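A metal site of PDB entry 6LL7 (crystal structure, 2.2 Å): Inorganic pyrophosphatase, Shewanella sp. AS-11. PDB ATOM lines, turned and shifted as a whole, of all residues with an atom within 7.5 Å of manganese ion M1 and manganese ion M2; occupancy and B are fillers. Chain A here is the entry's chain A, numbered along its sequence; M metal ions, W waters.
The side-chain carboxylate of Asp 73 sits close to the side-chain hydroxyl of Ser 16. The side-chain amide nitrogen (ND2) of Asn 118 lies within hydrogen-bond range of the side-chain carboxylate (OD1) of Asp 15, at 2.7 Å. The side-chain hydroxyl of Ser 117 lies close to the side-chain carboxylate of Asp 15, 2.9 Å away. OD1 of Asp 13 is in hydrogen-bond range of OG of Ser 16 (2.9 Å). The backbone carbonyl oxygen (O) of Ile 11 sits close to a ring nitrogen (ND1) of His 9 (3.5 Å). ND1 of His 95 sits at hydrogen-bond distance from O of Val 114 (3.0 Å). OD2 of Asp 147 lies close to SG of Cys 116 (3.2 Å). The side-chain carboxylate (OD1) of Asp 15 lies within hydrogen-bond range of the side-chain sulfur (SG) of Cys 116.
Of the 26 residues printed, 3 come within 4 Å of manganese ion M1.
Ser 117 touches manganese ion M2 (OG to MN, 3.97 Å). Within 4 Å of manganese ion M2: Asp 15, Asp 73, His 95, Ser 117 and Asp 147.
Water W1 is bound to manganese ion M1. Manganese ion M1 is bound by the side-chain carboxylate (OD2) of Asp 13. The side-chain carboxylate (OD2) of Asp 73 is bound to manganese ion M1. Manganese ion M1 is bound by a ring nitrogen (NE2) of His 9, 2.3 Å away.
OD1 of Asp 73 binds manganese ion M2, 2.1 Å away. The side-chain carboxylate (OD2) of Asp 15 is bound to manganese ion M2 (2.2 Å). NE2 of His 95 is bound to manganese ion M2 (2.2 Å). OD2 of Asp 147 is bound to manganese ion M2 (2.4 Å). Water W2 is bound to manganese ion M2 (2.4 Å).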
ATOM      1  N   HIS A   9     -19.639  -2.037   2.327  1.00  0.00           N
ATOM      2  CA  HIS A   9     -19.080  -3.402   2.570  1.00  0.00           C
ATOM      3  C   HIS A   9     -19.653  -4.410   1.556  1.00  0.00           C
ATOM      4  O   HIS A   9     -20.723  -4.165   0.974  1.00  0.00           O
ATOM      5  CB  HIS A   9     -19.307  -3.865   4.033  1.00  0.00           C
ATOM      6  CG  HIS A   9     -20.704  -3.766   4.548  1.00  0.00           C
ATOM      7  ND1 HIS A   9     -21.779  -4.434   3.978  1.00  0.00           N
ATOM      8  CD2 HIS A   9     -21.201  -3.117   5.631  1.00  0.00           C
ATOM      9  CE1 HIS A   9     -22.887  -4.153   4.650  1.00  0.00           C
ATOM     10  NE2 HIS A   9     -22.551  -3.364   5.686  1.00  0.00           N
ATOM     11  N   LYS A  10     -18.892  -5.485   1.365  1.00  0.00           N
ATOM     12  CA  LYS A  10     -19.344  -6.749   0.733  1.00  0.00           C
ATOM     13  C   LYS A  10     -20.705  -7.107   1.316  1.00  0.00           C
ATOM     14  O   LYS A  10     -20.868  -6.902   2.542  1.00  0.00           O
ATOM     15  CB  LYS A  10     -18.355  -7.885   1.009  1.00  0.00           C
ATOM     16  CG  LYS A  10     -16.941  -7.620   0.529  1.00  0.00           C
ATOM     17  CD  LYS A  10     -16.139  -8.893   0.323  1.00  0.00           C
ATOM     18  CE  LYS A  10     -15.157  -8.745  -0.820  1.00  0.00           C
ATOM     19  NZ  LYS A  10     -13.943  -9.563  -0.609  1.00  0.00           N
ATOM     20  N   ILE A  11     -21.597  -7.638   0.478  1.00  0.00           N
ATOM     21  CA  ILE A  11     -23.010  -7.951   0.827  1.00  0.00           C
ATOM     22  C   ILE A  11     -23.657  -6.659   1.299  1.00  0.00           C
ATOM     23  O   ILE A  11     -24.082  -6.529   2.439  1.00  0.00           O
ATOM     24  CB  ILE A  11     -23.077  -9.146   1.800  1.00  0.00           C
ATOM     25  CG1 ILE A  11     -22.283 -10.326   1.212  1.00  0.00           C
ATOM     26  CG2 ILE A  11     -24.523  -9.514   2.105  1.00  0.00           C
ATOM     27  CD1 ILE A  11     -22.469 -11.657   1.894  1.00  0.00           C
ATOM     28  N   PRO A  12     -23.725  -5.626   0.435  1.00  0.00           N
ATOM     29  CA  PRO A  12     -24.224  -4.311   0.847  1.00  0.00           C
ATOM     30  C   PRO A  12     -25.610  -4.318   1.491  1.00  0.00           C
ATOM     31  O   PRO A  12     -26.514  -4.940   0.978  1.00  0.00           O
ATOM     32  CB  PRO A  12     -24.264  -3.526  -0.485  1.00  0.00           C
ATOM     33  CG  PRO A  12     -24.183  -4.566  -1.571  1.00  0.00           C
ATOM     34  CD  PRO A  12     -23.333  -5.676  -0.981  1.00  0.00           C
ATOM     35  N   ASP A  13     -25.787  -3.590   2.580  1.00  0.00           N
ATOM     36  CA  ASP A  13     -27.112  -3.337   3.208  1.00  0.00           C
ATOM     37  C   ASP A  13     -27.573  -1.951   2.793  1.00  0.00           C
ATOM     38  O   ASP A  13     -26.845  -1.306   2.025  1.00  0.00           O
ATOM     39  CB  ASP A  13     -27.036  -3.472   4.738  1.00  0.00           C
ATOM     40  CG  ASP A  13     -25.924  -2.643   5.357  1.00  0.00           C
ATOM     41  OD1 ASP A  13     -25.273  -1.874   4.627  1.00  0.00           O
ATOM     42  OD2 ASP A  13     -25.700  -2.824   6.553  1.00  0.00           O
ATOM     43  N   SER A  14     -28.736  -1.477   3.285  1.00  0.00           N
ATOM     44  CA  SER A  14     -29.255  -0.127   2.926  1.00  0.00           C
ATOM     45  C   SER A  14     -28.244   0.971   3.292  1.00  0.00           C
ATOM     46  O   SER A  14     -28.032   1.881   2.433  1.00  0.00           O
ATOM     47  CB  SER A  14     -30.591   0.111   3.539  1.00  0.00           C
ATOM     48  OG  SER A  14     -31.579  -0.671   2.874  1.00  0.00           O
ATOM     49  N   ASP A  15     -27.601   0.878   4.471  1.00  0.00           N
ATOM     50  CA  ASP A  15     -26.628   1.876   4.960  1.00  0.00           C
ATOM     51  C   ASP A  15     -25.499   2.044   3.938  1.00  0.00           C
ATOM     52  O   ASP A  15     -25.203   3.207   3.586  1.00  0.00           O
ATOM     53  CB  ASP A  15     -26.054   1.510   6.339  1.00  0.00           C
ATOM     54  CG  ASP A  15     -25.321   2.645   7.040  1.00  0.00           C
ATOM     55  OD1 ASP A  15     -25.515   3.799   6.631  1.00  0.00           O
ATOM     56  OD2 ASP A  15     -24.589   2.359   8.030  1.00  0.00           O
ATOM     57  N   SER A  16     -24.872   0.926   3.520  1.00  0.00           N
ATOM     58  CA  SER A  16     -23.739   0.920   2.554  1.00  0.00           C
ATOM     59  C   SER A  16     -24.173   1.531   1.211  1.00  0.00           C
ATOM     60  O   SER A  16     -23.340   2.260   0.620  1.00  0.00           O
ATOM     61  CB  SER A  16     -23.179  -0.460   2.323  1.00  0.00           C
ATOM     62  OG  SER A  16     -22.744  -1.066   3.549  1.00  0.00           O
ATOM     63  N   VAL A  72     -17.441   3.307   3.282  1.00  0.00           N
ATOM     64  CA  VAL A  72     -18.680   3.534   4.099  1.00  0.00           C
ATOM     65  C   VAL A  72     -18.985   2.280   4.944  1.00  0.00           C
ATOM     66  O   VAL A  72     -18.947   1.161   4.381  1.00  0.00           O
ATOM     67  CB  VAL A  72     -19.867   3.884   3.210  1.00  0.00           C
ATOM     68  CG1 VAL A  72     -21.133   4.081   4.019  1.00  0.00           C
ATOM     69  CG2 VAL A  72     -19.569   5.092   2.342  1.00  0.00           C
ATOM     70  N   ASP A  73     -19.260   2.475   6.248  1.00  0.00           N
ATOM     71  CA  ASP A  73     -20.018   1.511   7.106  1.00  0.00           C
ATOM     72  C   ASP A  73     -19.155   0.299   7.464  1.00  0.00           C
ATOM     73  O   ASP A  73     -19.724  -0.774   7.739  1.00  0.00           O
ATOM     74  CB  ASP A  73     -21.290   1.037   6.388  1.00  0.00           C
ATOM     75  CG  ASP A  73     -22.352   0.379   7.261  1.00  0.00           C
ATOM     76  OD1 ASP A  73     -22.373   0.648   8.476  1.00  0.00           O
ATOM     77  OD2 ASP A  73     -23.144  -0.401   6.684  1.00  0.00           O
ATOM     78  N   HIS A  74     -17.851   0.438   7.407  1.00  0.00           N
ATOM     79  CA  HIS A  74     -16.882  -0.519   8.022  1.00  0.00           C
ATOM     80  C   HIS A  74     -15.495   0.146   8.104  1.00  0.00           C
ATOM     81  O   HIS A  74     -15.329   1.225   7.531  1.00  0.00           O
ATOM     82  CB  HIS A  74     -16.838  -1.827   7.232  1.00  0.00           C
ATOM     83  CG  HIS A  74     -16.243  -1.674   5.871  1.00  0.00           C
ATOM     84  ND1 HIS A  74     -14.895  -1.941   5.639  1.00  0.00           N
ATOM     85  CD2 HIS A  74     -16.776  -1.327   4.683  1.00  0.00           C
ATOM     86  CE1 HIS A  74     -14.647  -1.734   4.367  1.00  0.00           C
ATOM     87  NE2 HIS A  74     -15.773  -1.371   3.753  1.00  0.00           N
ATOM     88  N   GLN A  79     -14.161  -6.853   4.807  1.00  0.00           N
ATOM     89  CA  GLN A  79     -15.385  -6.235   4.248  1.00  0.00           C
ATOM     90  C   GLN A  79     -15.056  -5.272   3.112  1.00  0.00           C
ATOM     91  O   GLN A  79     -15.988  -4.822   2.435  1.00  0.00           O
ATOM     92  CB  GLN A  79     -16.169  -5.547   5.362  1.00  0.00           C
ATOM     93  CG  GLN A  79     -17.032  -6.525   6.159  1.00  0.00           C
ATOM     94  CD  GLN A  79     -17.974  -5.792   7.082  1.00  0.00           C
ATOM     95  OE1 GLN A  79     -19.155  -5.607   6.787  1.00  0.00           O
ATOM     96  NE2 GLN A  79     -17.432  -5.364   8.214  1.00  0.00           N
ATOM     97  N   ASP A  94     -18.098   5.852   9.124  1.00  0.00           N
ATOM     98  CA  ASP A  94     -18.560   4.602   9.774  1.00  0.00           C
ATOM     99  C   ASP A  94     -19.039   4.888  11.202  1.00  0.00           C
ATOM    100  O   ASP A  94     -18.861   6.018  11.696  1.00  0.00           O
ATOM    101  CB  ASP A  94     -17.427   3.569   9.767  1.00  0.00           C
ATOM    102  CG  ASP A  94     -17.838   2.189  10.240  1.00  0.00           C
ATOM    103  OD1 ASP A  94     -19.067   1.902  10.232  1.00  0.00           O
ATOM    104  OD2 ASP A  94     -16.929   1.399  10.605  1.00  0.00           O
ATOM    105  N   HIS A  95     -19.602   3.857  11.839  1.00  0.00           N
ATOM    106  CA  HIS A  95     -20.094   3.886  13.236  1.00  0.00           C
ATOM    107  C   HIS A  95     -19.746   2.562  13.909  1.00  0.00           C
ATOM    108  O   HIS A  95     -20.468   2.180  14.848  1.00  0.00           O
ATOM    109  CB  HIS A  95     -21.603   4.143  13.255  1.00  0.00           C
ATOM    110  CG  HIS A  95     -22.417   3.118  12.541  1.00  0.00           C
ATOM    111  ND1 HIS A  95     -23.216   2.205  13.202  1.00  0.00           N
ATOM    112  CD2 HIS A  95     -22.540   2.841  11.224  1.00  0.00           C
ATOM    113  CE1 HIS A  95     -23.807   1.419  12.319  1.00  0.00           C
ATOM    114  NE2 HIS A  95     -23.408   1.800  11.090  1.00  0.00           N
ATOM    115  N   HIS A  96     -18.682   1.882  13.469  1.00  0.00           N
ATOM    116  CA  HIS A  96     -18.183   0.635  14.104  1.00  0.00           C
ATOM    117  C   HIS A  96     -16.870   0.903  14.830  1.00  0.00           C
ATOM    118  O   HIS A  96     -16.277   2.000  14.671  1.00  0.00           O
ATOM    119  CB  HIS A  96     -17.975  -0.468  13.074  1.00  0.00           C
ATOM    120  CG  HIS A  96     -19.257  -0.888  12.435  1.00  0.00           C
ATOM    121  ND1 HIS A  96     -19.716  -0.340  11.247  1.00  0.00           N
ATOM    122  CD2 HIS A  96     -20.186  -1.805  12.820  1.00  0.00           C
ATOM    123  CE1 HIS A  96     -20.878  -0.884  10.940  1.00  0.00           C
ATOM    124  NE2 HIS A  96     -21.166  -1.802  11.887  1.00  0.00           N
ATOM    125  N   VAL A 114     -22.535   5.855  16.895  1.00  0.00           N
ATOM    126  CA  VAL A 114     -23.976   6.000  16.581  1.00  0.00           C
ATOM    127  C   VAL A 114     -24.424   4.703  15.900  1.00  0.00           C
ATOM    128  O   VAL A 114     -23.578   3.774  15.787  1.00  0.00           O
ATOM    129  CB  VAL A 114     -24.256   7.240  15.720  1.00  0.00           C
ATOM    130  CG1 VAL A 114     -23.932   8.503  16.487  1.00  0.00           C
ATOM    131  CG2 VAL A 114     -23.509   7.210  14.391  1.00  0.00           C
ATOM    132  N   GLY A 115     -25.691   4.626  15.523  1.00  0.00           N
ATOM    133  CA  GLY A 115     -26.318   3.407  14.991  1.00  0.00           C
ATOM    134  C   GLY A 115     -26.290   3.312  13.473  1.00  0.00           C
ATOM    135  O   GLY A 115     -26.768   2.277  12.953  1.00  0.00           O
ATOM    136  N   CYS A 116     -25.753   4.321  12.773  1.00  0.00           N
ATOM    137  CA  CYS A 116     -25.839   4.403  11.296  1.00  0.00           C
ATOM    138  C   CYS A 116     -24.853   5.397  10.670  1.00  0.00           C
ATOM    139  O   CYS A 116     -24.861   6.590  11.065  1.00  0.00           O
ATOM    140  CB  CYS A 116     -27.250   4.794  10.893  1.00  0.00           C
ATOM    141  SG  CYS A 116     -27.626   4.457   9.156  1.00  0.00           S
ATOM    142  N   SER A 117     -24.120   4.950   9.642  1.00  0.00           N
ATOM    143  CA  SER A 117     -23.180   5.774   8.844  1.00  0.00           C
ATOM    144  C   SER A 117     -23.897   7.011   8.299  1.00  0.00           C
ATOM    145  O   SER A 117     -23.314   8.101   8.261  1.00  0.00           O
ATOM    146  CB  SER A 117     -22.533   4.972   7.748  1.00  0.00           C
ATOM    147  OG  SER A 117     -22.062   3.716   8.203  1.00  0.00           O
ATOM    148  N   ASN A 118     -25.161   6.851   7.923  1.00  0.00           N
ATOM    149  CA  ASN A 118     -25.963   7.920   7.282  1.00  0.00           C
ATOM    150  C   ASN A 118     -26.218   9.040   8.314  1.00  0.00           C
ATOM    151  O   ASN A 118     -26.410  10.164   7.919  1.00  0.00           O
ATOM    152  CB  ASN A 118     -27.203   7.322   6.615  1.00  0.00           C
ATOM    153  CG  ASN A 118     -26.942   6.948   5.183  1.00  0.00           C
ATOM    154  OD1 ASN A 118     -27.198   7.742   4.275  1.00  0.00           O
ATOM    155  ND2 ASN A 118     -26.411   5.757   4.932  1.00  0.00           N
ATOM    156  N   ALA A 143     -32.142   4.406   5.565  1.00  0.00           N
ATOM    157  CA  ALA A 143     -30.895   3.735   5.987  1.00  0.00           C
ATOM    158  C   ALA A 143     -30.839   3.709   7.518  1.00  0.00           C
ATOM    159  O   ALA A 143     -30.468   2.649   8.070  1.00  0.00           O
ATOM    160  CB  ALA A 143     -29.686   4.414   5.424  1.00  0.00           C
ATOM    161  N   ASP A 147     -30.977   0.357   9.875  1.00  0.00           N
ATOM    162  CA  ASP A 147     -29.869   0.058  10.802  1.00  0.00           C
ATOM    163  C   ASP A 147     -30.367  -0.018  12.249  1.00  0.00           C
ATOM    164  O   ASP A 147     -29.921  -0.941  12.969  1.00  0.00           O
ATOM    165  CB  ASP A 147     -28.746   1.113  10.707  1.00  0.00           C
ATOM    166  CG  ASP A 147     -27.470   0.642  10.010  1.00  0.00           C
ATOM    167  OD1 ASP A 147     -27.388  -0.572   9.776  1.00  0.00           O
ATOM    168  OD2 ASP A 147     -26.552   1.498   9.733  1.00  0.00           O
ATOM    169  N   ASP A 202     -27.994 -11.263   4.347  1.00  0.00           N
ATOM    170  CA  ASP A 202     -27.060 -10.537   5.249  1.00  0.00           C
ATOM    171  C   ASP A 202     -26.262 -11.567   6.065  1.00  0.00           C
ATOM    172  O   ASP A 202     -26.575 -11.756   7.260  1.00  0.00           O
ATOM    173  CB  ASP A 202     -27.813  -9.577   6.174  1.00  0.00           C
ATOM    174  CG  ASP A 202     -26.890  -8.762   7.055  1.00  0.00           C
ATOM    175  OD1 ASP A 202     -25.801  -8.398   6.577  1.00  0.00           O
ATOM    176  OD2 ASP A 202     -27.245  -8.525   8.231  1.00  0.00           O
ATOM    177  N   LYS A 204     -22.335 -13.052   7.299  1.00  0.00           N
ATOM    178  CA  LYS A 204     -20.937 -12.685   7.634  1.00  0.00           C
ATOM    179  C   LYS A 204     -20.204 -13.883   8.222  1.00  0.00           C
ATOM    180  O   LYS A 204     -20.825 -14.653   8.975  1.00  0.00           O
ATOM    181  CB  LYS A 204     -20.920 -11.545   8.643  1.00  0.00           C
ATOM    182  CG  LYS A 204     -21.154 -10.161   8.063  1.00  0.00           C
ATOM    183  CD  LYS A 204     -21.030  -9.110   9.146  1.00  0.00           C
ATOM    184  CE  LYS A 204     -21.174  -7.694   8.629  1.00  0.00           C
ATOM    185  NZ  LYS A 204     -20.673  -6.710   9.605  1.00  0.00           N
ATOM    186  N   ARG A 294     -27.047  -8.226  15.700  1.00  0.00           N
ATOM    187  CA  ARG A 294     -25.970  -9.241  15.581  1.00  0.00           C
ATOM    188  C   ARG A 294     -24.700  -8.727  16.261  1.00  0.00           C
ATOM    189  O   ARG A 294     -24.096  -9.484  17.034  1.00  0.00           O
ATOM    190  CB  ARG A 294     -25.681  -9.598  14.116  1.00  0.00           C
ATOM    191  CG  ARG A 294     -24.580 -10.649  13.974  1.00  0.00           C
ATOM    192  CD  ARG A 294     -24.460 -11.222  12.573  1.00  0.00           C
ATOM    193  NE  ARG A 294     -24.357 -10.153  11.598  1.00  0.00           N
ATOM    194  CZ  ARG A 294     -24.744 -10.227  10.322  1.00  0.00           C
ATOM    195  NH1 ARG A 294     -25.247 -11.333   9.798  1.00  0.00           N
ATOM    196  NH2 ARG A 294     -24.601  -9.177   9.537  1.00  0.00           N
ATOM    197  N   LYS A 295     -24.280  -7.480  15.985  1.00  0.00           N
ATOM    198  CA  LYS A 295     -22.936  -6.988  16.424  1.00  0.00           C
ATOM    199  C   LYS A 295     -22.944  -6.679  17.925  1.00  0.00           C
ATOM    200  O   LYS A 295     -21.848  -6.613  18.494  1.00  0.00           O
ATOM    201  CB  LYS A 295     -22.436  -5.811  15.573  1.00  0.00           C
ATOM    202  CG  LYS A 295     -23.078  -4.454  15.833  1.00  0.00           C
ATOM    203  CD  LYS A 295     -22.153  -3.275  15.685  1.00  0.00           C
ATOM    204  CE  LYS A 295     -22.884  -1.947  15.734  1.00  0.00           C
ATOM    205  NZ  LYS A 295     -23.893  -1.857  14.638  1.00  0.00           N
HETATM  206 MN    MN M   1     -23.864  -2.396   7.240  1.00  0.00          MN
HETATM  207 MN    MN M   2     -24.313   0.662   9.374  1.00  0.00          MN
HETATM  208  O   HOH W   1     -22.672  -2.201   8.681  1.00  0.00           O
HETATM  209  O   HOH W   2     -24.632  -1.655  10.023  1.00  0.00           O
